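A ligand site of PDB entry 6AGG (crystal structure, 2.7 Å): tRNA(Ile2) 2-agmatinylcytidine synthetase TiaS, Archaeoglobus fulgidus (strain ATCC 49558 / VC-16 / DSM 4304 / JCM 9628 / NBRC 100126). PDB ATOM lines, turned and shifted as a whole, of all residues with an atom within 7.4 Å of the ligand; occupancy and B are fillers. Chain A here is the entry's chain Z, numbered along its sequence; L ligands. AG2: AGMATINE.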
ATOM      1  N   GLU A 159     -35.451  -7.570  14.835  1.00  0.00           N
ATOM      2  CA  GLU A 159     -34.016  -7.324  14.787  1.00  0.00           C
ATOM      3  C   GLU A 159     -33.498  -7.417  13.359  1.00  0.00           C
ATOM      4  O   GLU A 159     -33.738  -8.406  12.649  1.00  0.00           O
ATOM      5  CB  GLU A 159     -33.233  -8.229  15.724  1.00  0.00           C
ATOM      6  CG  GLU A 159     -31.855  -7.668  16.083  1.00  0.00           C
ATOM      7  CD  GLU A 159     -31.162  -8.464  17.185  1.00  0.00           C
ATOM      8  OE1 GLU A 159     -31.785  -9.399  17.717  1.00  0.00           O
ATOM      9  OE2 GLU A 159     -30.001  -8.135  17.515  1.00  0.00           O
ATOM     10  N   LEU A 160     -32.832  -6.358  12.928  1.00  0.00           N
ATOM     11  CA  LEU A 160     -32.198  -6.331  11.650  1.00  0.00           C
ATOM     12  C   LEU A 160     -30.770  -6.833  11.883  1.00  0.00           C
ATOM     13  O   LEU A 160     -29.940  -6.124  12.442  1.00  0.00           O
ATOM     14  CB  LEU A 160     -32.251  -4.909  11.070  1.00  0.00           C
ATOM     15  CG  LEU A 160     -31.591  -4.645   9.716  1.00  0.00           C
ATOM     16  CD1 LEU A 160     -32.444  -3.710   8.869  1.00  0.00           C
ATOM     17  CD2 LEU A 160     -30.201  -4.081   9.911  1.00  0.00           C
ATOM     18  N   ILE A 161     -30.530  -8.084  11.512  1.00  0.00           N
ATOM     19  CA  ILE A 161     -29.205  -8.675  11.633  1.00  0.00           C
ATOM     20  C   ILE A 161     -28.404  -8.406  10.373  1.00  0.00           C
ATOM     21  O   ILE A 161     -28.769  -8.871   9.295  1.00  0.00           O
ATOM     22  CB  ILE A 161     -29.253 -10.208  11.829  1.00  0.00           C
ATOM     23  CG1 ILE A 161     -30.221 -10.601  12.960  1.00  0.00           C
ATOM     24  CG2 ILE A 161     -27.843 -10.740  12.072  1.00  0.00           C
ATOM     25  CD1 ILE A 161     -29.569 -10.721  14.336  1.00  0.00           C
ATOM     26  N   PHE A 192     -34.264   0.592  19.612  1.00  0.00           N
ATOM     27  CA  PHE A 192     -33.974   0.698  21.035  1.00  0.00           C
ATOM     28  C   PHE A 192     -32.925  -0.335  21.417  1.00  0.00           C
ATOM     29  O   PHE A 192     -32.727  -1.308  20.704  1.00  0.00           O
ATOM     30  CB  PHE A 192     -35.255   0.468  21.837  1.00  0.00           C
ATOM     31  CG  PHE A 192     -35.762  -0.940  21.723  1.00  0.00           C
ATOM     32  CD1 PHE A 192     -35.400  -1.901  22.665  1.00  0.00           C
ATOM     33  CD2 PHE A 192     -36.587  -1.321  20.670  1.00  0.00           C
ATOM     34  CE1 PHE A 192     -35.850  -3.199  22.561  1.00  0.00           C
ATOM     35  CE2 PHE A 192     -37.045  -2.623  20.561  1.00  0.00           C
ATOM     36  CZ  PHE A 192     -36.666  -3.569  21.506  1.00  0.00           C
ATOM     37  N   ASP A 193     -32.280  -0.118  22.555  1.00  0.00           N
ATOM     38  CA  ASP A 193     -31.298  -1.068  23.104  1.00  0.00           C
ATOM     39  C   ASP A 193     -30.134  -1.366  22.171  1.00  0.00           C
ATOM     40  O   ASP A 193     -29.481  -2.404  22.297  1.00  0.00           O
ATOM     41  CB  ASP A 193     -31.971  -2.387  23.494  1.00  0.00           C
ATOM     42  CG  ASP A 193     -32.463  -2.383  24.929  1.00  0.00           C
ATOM     43  OD1 ASP A 193     -32.061  -1.483  25.687  1.00  0.00           O
ATOM     44  OD2 ASP A 193     -33.262  -3.272  25.284  1.00  0.00           O
ATOM     45  N   ASN A 194     -29.868  -0.467  21.242  1.00  0.00           N
ATOM     46  CA  ASN A 194     -28.799  -0.653  20.277  1.00  0.00           C
ATOM     47  C   ASN A 194     -27.532   0.101  20.650  1.00  0.00           C
ATOM     48  O   ASN A 194     -26.542   0.073  19.938  1.00  0.00           O
ATOM     49  CB  ASN A 194     -29.279  -0.244  18.898  1.00  0.00           C
ATOM     50  CG  ASN A 194     -30.467  -1.061  18.443  1.00  0.00           C
ATOM     51  OD1 ASN A 194     -30.547  -2.265  18.712  1.00  0.00           O
ATOM     52  ND2 ASN A 194     -31.397  -0.419  17.755  1.00  0.00           N
ATOM     53  N   VAL A 195     -27.579   0.770  21.791  1.00  0.00           N
ATOM     54  CA  VAL A 195     -26.427   1.511  22.278  1.00  0.00           C
ATOM     55  C   VAL A 195     -26.661   1.912  23.735  1.00  0.00           C
ATOM     56  O   VAL A 195     -27.804   2.035  24.177  1.00  0.00           O
ATOM     57  CB  VAL A 195     -26.122   2.753  21.398  1.00  0.00           C
ATOM     58  CG1 VAL A 195     -27.313   3.689  21.336  1.00  0.00           C
ATOM     59  CG2 VAL A 195     -24.900   3.472  21.911  1.00  0.00           C
ATOM     60  N   VAL A 202     -21.189   1.127  22.448  1.00  0.00           N
ATOM     61  CA  VAL A 202     -22.093   0.547  21.465  1.00  0.00           C
ATOM     62  C   VAL A 202     -22.453  -0.866  21.910  1.00  0.00           C
ATOM     63  O   VAL A 202     -21.650  -1.533  22.557  1.00  0.00           O
ATOM     64  CB  VAL A 202     -21.456   0.476  20.072  1.00  0.00           C
ATOM     65  CG1 VAL A 202     -22.456  -0.063  19.051  1.00  0.00           C
ATOM     66  CG2 VAL A 202     -20.954   1.859  19.665  1.00  0.00           C
ATOM     67  N   VAL A 203     -23.658  -1.306  21.569  1.00  0.00           N
ATOM     68  CA  VAL A 203     -24.201  -2.502  22.189  1.00  0.00           C
ATOM     69  C   VAL A 203     -24.721  -3.535  21.189  1.00  0.00           C
ATOM     70  O   VAL A 203     -24.843  -4.707  21.522  1.00  0.00           O
ATOM     71  CB  VAL A 203     -25.306  -2.121  23.210  1.00  0.00           C
ATOM     72  CG1 VAL A 203     -26.122  -3.330  23.606  1.00  0.00           C
ATOM     73  CG2 VAL A 203     -24.681  -1.484  24.434  1.00  0.00           C
ATOM     74  N   CYS A 204     -25.023  -3.096  19.969  1.00  0.00           N
ATOM     75  CA  CYS A 204     -25.569  -3.995  18.954  1.00  0.00           C
ATOM     76  C   CYS A 204     -24.465  -4.717  18.167  1.00  0.00           C
ATOM     77  O   CYS A 204     -24.728  -5.357  17.155  1.00  0.00           O
ATOM     78  CB  CYS A 204     -26.477  -3.221  17.991  1.00  0.00           C
ATOM     79  SG  CYS A 204     -25.792  -1.655  17.399  1.00  0.00           S
ATOM     80  N   ILE A 205     -23.237  -4.613  18.658  1.00  0.00           N
ATOM     81  CA  ILE A 205     -22.101  -5.163  17.934  1.00  0.00           C
ATOM     82  C   ILE A 205     -21.369  -6.237  18.732  1.00  0.00           C
ATOM     83  O   ILE A 205     -20.738  -5.964  19.750  1.00  0.00           O
ATOM     84  CB  ILE A 205     -21.120  -4.053  17.529  1.00  0.00           C
ATOM     85  CG1 ILE A 205     -21.791  -3.129  16.502  1.00  0.00           C
ATOM     86  CG2 ILE A 205     -19.849  -4.644  16.986  1.00  0.00           C
ATOM     87  CD1 ILE A 205     -20.887  -2.052  15.960  1.00  0.00           C
ATOM     88  N   PRO A 206     -21.450  -7.492  18.250  1.00  0.00           N
ATOM     89  CA  PRO A 206     -20.845  -8.619  18.945  1.00  0.00           C
ATOM     90  C   PRO A 206     -19.323  -8.488  19.047  1.00  0.00           C
ATOM     91  O   PRO A 206     -18.683  -7.800  18.244  1.00  0.00           O
ATOM     92  CB  PRO A 206     -21.222  -9.822  18.067  1.00  0.00           C
ATOM     93  CG  PRO A 206     -21.479  -9.248  16.715  1.00  0.00           C
ATOM     94  CD  PRO A 206     -22.048  -7.883  16.961  1.00  0.00           C
ATOM     95  N   TYR A 214     -23.729  -6.416  12.913  1.00  0.00           N
ATOM     96  CA  TYR A 214     -24.557  -5.831  13.948  1.00  0.00           C
ATOM     97  C   TYR A 214     -25.951  -6.421  13.878  1.00  0.00           C
ATOM     98  O   TYR A 214     -26.423  -6.830  12.808  1.00  0.00           O
ATOM     99  CB  TYR A 214     -24.606  -4.304  13.829  1.00  0.00           C
ATOM    100  CG  TYR A 214     -25.170  -3.804  12.518  1.00  0.00           C
ATOM    101  CD1 TYR A 214     -24.341  -3.285  11.537  1.00  0.00           C
ATOM    102  CD2 TYR A 214     -26.535  -3.862  12.253  1.00  0.00           C
ATOM    103  CE1 TYR A 214     -24.840  -2.828  10.335  1.00  0.00           C
ATOM    104  CE2 TYR A 214     -27.042  -3.409  11.047  1.00  0.00           C
ATOM    105  CZ  TYR A 214     -26.191  -2.894  10.093  1.00  0.00           C
ATOM    106  OH  TYR A 214     -26.681  -2.426   8.890  1.00  0.00           O
ATOM    107  N   GLY A 215     -26.610  -6.473  15.033  1.00  0.00           N
ATOM    108  CA  GLY A 215     -28.018  -6.813  15.127  1.00  0.00           C
ATOM    109  C   GLY A 215     -28.738  -5.650  15.785  1.00  0.00           C
ATOM    110  O   GLY A 215     -28.477  -5.318  16.945  1.00  0.00           O
ATOM    111  N   ILE A 216     -29.615  -5.005  15.029  1.00  0.00           N
ATOM    112  CA  ILE A 216     -30.312  -3.819  15.531  1.00  0.00           C
ATOM    113  C   ILE A 216     -31.770  -4.103  15.886  1.00  0.00           C
ATOM    114  O   ILE A 216     -32.541  -4.550  15.038  1.00  0.00           O
ATOM    115  CB  ILE A 216     -30.249  -2.674  14.503  1.00  0.00           C
ATOM    116  CG1 ILE A 216     -28.843  -2.053  14.488  1.00  0.00           C
ATOM    117  CG2 ILE A 216     -31.264  -1.594  14.822  1.00  0.00           C
ATOM    118  CD1 ILE A 216     -28.524  -1.306  13.203  1.00  0.00           C
ATOM    119  N   ARG A 217     -32.127  -3.851  17.144  1.00  0.00           N
ATOM    120  CA  ARG A 217     -33.499  -4.084  17.627  1.00  0.00           C
ATOM    121  C   ARG A 217     -34.421  -2.860  17.509  1.00  0.00           C
ATOM    122  O   ARG A 217     -34.019  -1.727  17.771  1.00  0.00           O
ATOM    123  CB  ARG A 217     -33.465  -4.595  19.064  1.00  0.00           C
ATOM    124  CG  ARG A 217     -33.160  -6.074  19.184  1.00  0.00           C
ATOM    125  CD  ARG A 217     -32.188  -6.318  20.322  1.00  0.00           C
ATOM    126  NE  ARG A 217     -32.116  -7.720  20.696  1.00  0.00           N
ATOM    127  CZ  ARG A 217     -31.329  -8.208  21.642  1.00  0.00           C
ATOM    128  NH1 ARG A 217     -30.523  -7.403  22.310  1.00  0.00           N
ATOM    129  NH2 ARG A 217     -31.341  -9.497  21.924  1.00  0.00           N
ATOM    130  N   GLY A 218     -35.670  -3.121  17.126  1.00  0.00           N
ATOM    131  CA  GLY A 218     -36.605  -2.061  16.786  1.00  0.00           C
ATOM    132  C   GLY A 218     -38.050  -2.510  16.735  1.00  0.00           C
ATOM    133  O   GLY A 218     -38.403  -3.595  17.210  1.00  0.00           O
ATOM    134  N   HIS A 246     -37.293 -10.998  21.698  1.00  0.00           N
ATOM    135  CA  HIS A 246     -36.434 -10.074  22.416  1.00  0.00           C
ATOM    136  C   HIS A 246     -37.281  -9.026  23.098  1.00  0.00           C
ATOM    137  O   HIS A 246     -38.209  -8.518  22.486  1.00  0.00           O
ATOM    138  CB  HIS A 246     -35.506  -9.351  21.450  1.00  0.00           C
ATOM    139  CG  HIS A 246     -34.540 -10.235  20.739  1.00  0.00           C
ATOM    140  ND1 HIS A 246     -33.957 -11.322  21.340  1.00  0.00           N
ATOM    141  CD2 HIS A 246     -34.060 -10.196  19.476  1.00  0.00           C
ATOM    142  CE1 HIS A 246     -33.148 -11.912  20.480  1.00  0.00           C
ATOM    143  NE2 HIS A 246     -33.188 -11.248  19.344  1.00  0.00           N
ATOM    144  N   PRO A 397     -28.596  -1.184  32.772  1.00  0.00           N
ATOM    145  CA  PRO A 397     -28.311  -0.400  31.573  1.00  0.00           C
ATOM    146  C   PRO A 397     -28.278  -1.319  30.356  1.00  0.00           C
ATOM    147  O   PRO A 397     -28.050  -2.513  30.508  1.00  0.00           O
ATOM    148  CB  PRO A 397     -26.933   0.188  31.871  1.00  0.00           C
ATOM    149  CG  PRO A 397     -26.286  -0.850  32.719  1.00  0.00           C
ATOM    150  CD  PRO A 397     -27.365  -1.509  33.515  1.00  0.00           C
ATOM    151  N   PRO A 398     -28.506  -0.753  29.166  1.00  0.00           N
ATOM    152  CA  PRO A 398     -28.651  -1.548  27.939  1.00  0.00           C
ATOM    153  C   PRO A 398     -27.490  -2.522  27.693  1.00  0.00           C
ATOM    154  O   PRO A 398     -27.681  -3.563  27.065  1.00  0.00           O
ATOM    155  CB  PRO A 398     -28.701  -0.478  26.843  1.00  0.00           C
ATOM    156  CG  PRO A 398     -29.188   0.756  27.542  1.00  0.00           C
ATOM    157  CD  PRO A 398     -28.580   0.693  28.905  1.00  0.00           C
ATOM    158  N   SER A 399     -26.311  -2.192  28.196  1.00  0.00           N
ATOM    159  CA  SER A 399     -25.140  -3.044  27.985  1.00  0.00           C
ATOM    160  C   SER A 399     -25.203  -4.290  28.866  1.00  0.00           C
ATOM    161  O   SER A 399     -24.385  -5.211  28.744  1.00  0.00           O
ATOM    162  CB  SER A 399     -23.854  -2.252  28.220  1.00  0.00           C
ATOM    163  OG  SER A 399     -22.966  -2.917  29.093  1.00  0.00           O
ATOM    164  N   ALA A 400     -26.198  -4.323  29.752  1.00  0.00           N
ATOM    165  CA  ALA A 400     -26.386  -5.444  30.660  1.00  0.00           C
ATOM    166  C   ALA A 400     -27.695  -6.172  30.375  1.00  0.00           C
ATOM    167  O   ALA A 400     -28.017  -7.156  31.030  1.00  0.00           O
ATOM    168  CB  ALA A 400     -26.348  -4.976  32.098  1.00  0.00           C
ATOM    169  N   ARG A 401     -28.446  -5.670  29.402  1.00  0.00           N
ATOM    170  CA  ARG A 401     -29.758  -6.240  29.085  1.00  0.00           C
ATOM    171  C   ARG A 401     -29.658  -7.681  28.572  1.00  0.00           C
ATOM    172  O   ARG A 401     -28.764  -8.031  27.784  1.00  0.00           O
ATOM    173  CB  ARG A 401     -30.524  -5.385  28.077  1.00  0.00           C
ATOM    174  CG  ARG A 401     -31.963  -5.859  27.813  1.00  0.00           C
ATOM    175  CD  ARG A 401     -33.000  -4.740  28.038  1.00  0.00           C
ATOM    176  NE  ARG A 401     -32.818  -4.080  29.327  1.00  0.00           N
ATOM    177  CZ  ARG A 401     -32.379  -2.837  29.489  1.00  0.00           C
ATOM    178  NH1 ARG A 401     -32.068  -2.088  28.436  1.00  0.00           N
ATOM    179  NH2 ARG A 401     -32.250  -2.342  30.720  1.00  0.00           N
ATOM    180  N   ARG A 402     -30.579  -8.508  29.035  1.00  0.00           N
ATOM    181  CA  ARG A 402     -30.680  -9.871  28.563  1.00  0.00           C
ATOM    182  C   ARG A 402     -31.712  -9.944  27.451  1.00  0.00           C
ATOM    183  O   ARG A 402     -32.751  -9.281  27.530  1.00  0.00           O
ATOM    184  CB  ARG A 402     -30.997 -10.825  29.715  1.00  0.00           C
ATOM    185  CG  ARG A 402     -29.861 -10.898  30.728  1.00  0.00           C
ATOM    186  CD  ARG A 402     -30.132 -11.879  31.867  1.00  0.00           C
ATOM    187  NE  ARG A 402     -29.845 -13.263  31.498  1.00  0.00           N
ATOM    188  CZ  ARG A 402     -29.712 -14.256  32.383  1.00  0.00           C
ATOM    189  NH1 ARG A 402     -29.831 -14.008  33.689  1.00  0.00           N
ATOM    190  NH2 ARG A 402     -29.449 -15.484  31.979  1.00  0.00           N
ATOM    191  N   HIS A 403     -31.406 -10.698  26.404  1.00  0.00           N
ATOM    192  CA  HIS A 403     -32.247 -10.801  25.211  1.00  0.00           C
ATOM    193  C   HIS A 403     -33.763 -10.736  25.522  1.00  0.00           C
ATOM    194  O   HIS A 403     -34.482  -9.937  24.927  1.00  0.00           O
ATOM    195  CB  HIS A 403     -31.899 -12.069  24.415  1.00  0.00           C
ATOM    196  CG  HIS A 403     -30.450 -12.195  24.074  1.00  0.00           C
ATOM    197  ND1 HIS A 403     -29.786 -11.306  23.246  1.00  0.00           N
ATOM    198  CD2 HIS A 403     -29.519 -13.125  24.427  1.00  0.00           C
ATOM    199  CE1 HIS A 403     -28.526 -11.670  23.119  1.00  0.00           C
ATOM    200  NE2 HIS A 403     -28.339 -12.774  23.819  1.00  0.00           N
HETATM  201  N   AG2 L   1     -24.871  -7.734  26.217  1.00  0.00           N
HETATM  202  CA  AG2 L   1     -25.831  -6.788  25.696  1.00  0.00           C
HETATM  203  CB  AG2 L   1     -26.366  -7.048  24.333  1.00  0.00           C
HETATM  204  CG  AG2 L   1     -27.521  -6.244  23.844  1.00  0.00           C
HETATM  205  CD  AG2 L   1     -27.843  -6.296  22.390  1.00  0.00           C
HETATM  206  NE  AG2 L   1     -28.286  -5.099  21.729  1.00  0.00           N
HETATM  207  CZ  AG2 L   1     -28.624  -5.139  20.333  1.00  0.00           C
HETATM  208  NH1 AG2 L   1     -28.529  -6.254  19.646  1.00  0.00           N
HETATM  209  NH2 AG2 L   1     -29.027  -4.044  19.742  1.00  0.00           N
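The side-chain amide oxygen (OD1) of Asn 194 lies within hydrogen-bond range of a nitrogen (NH2) of the ligand (2.6 Å).
O of Gly 215 is in hydrogen-bond range of NH1 of the ligand (2.9 Å).
A nitrogen (NE) of the ligand sits at hydrogen-bond distance from the backbone carbonyl oxygen (O) of Asp 193 (3.0 Å).
OE2 of Glu 159 is in salt-bridge range of NH1 of the ligand.
A nitrogen (NE) of the ligand lies close to the backbone carbonyl oxygen (O) of Val 203, 3.5 Å away.
OD1 of Asn 194 is in hydrogen-bond range of N of Arg 217 (2.7 Å).
The side-chain sulfur of Cys 204 sits at hydrogen-bond distance from the backbone carbonyl oxygen of Asn 194, 3.2 Å away.
OD1 of Asn 194 lies close to O of Phe 192 (3.1 Å).
The guanidinium group (NE) of Arg 217 is in salt-bridge range of the side-chain carboxylate (OE1) of Glu 159 (3.4 Å).
N of Phe 192 sits at hydrogen-bond distance from O of Arg 217 (3.0 Å).
A ring nitrogen (ND1) of His 403 is in hydrogen-bond range of the guanidinium group (NH2) of Arg 217 (2.7 Å).
A ring nitrogen (ND1) of His 246 is in hydrogen-bond range of the guanidinium group (NH2) of Arg 217 (3.2 Å).
OE1 of Glu 159 lies within hydrogen-bond range of NE2 of His 246, at 2.8 Å.
NH1 of Arg 217 sits close to NE of the ligand (3.3 Å).
CB of Cys 204 touches NH2 of the ligand, at 3.2 Å.
Pro 398 touches the ligand (O to CA, 3.96 Å).
Ser 399 touches the ligand (O to N, 3.6 Å).
O of Arg 401 touches CA of the ligand, at 3.8 Å.
The nearest printed residue that does not touch the ligand is Ile 216 (4.4 Å).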
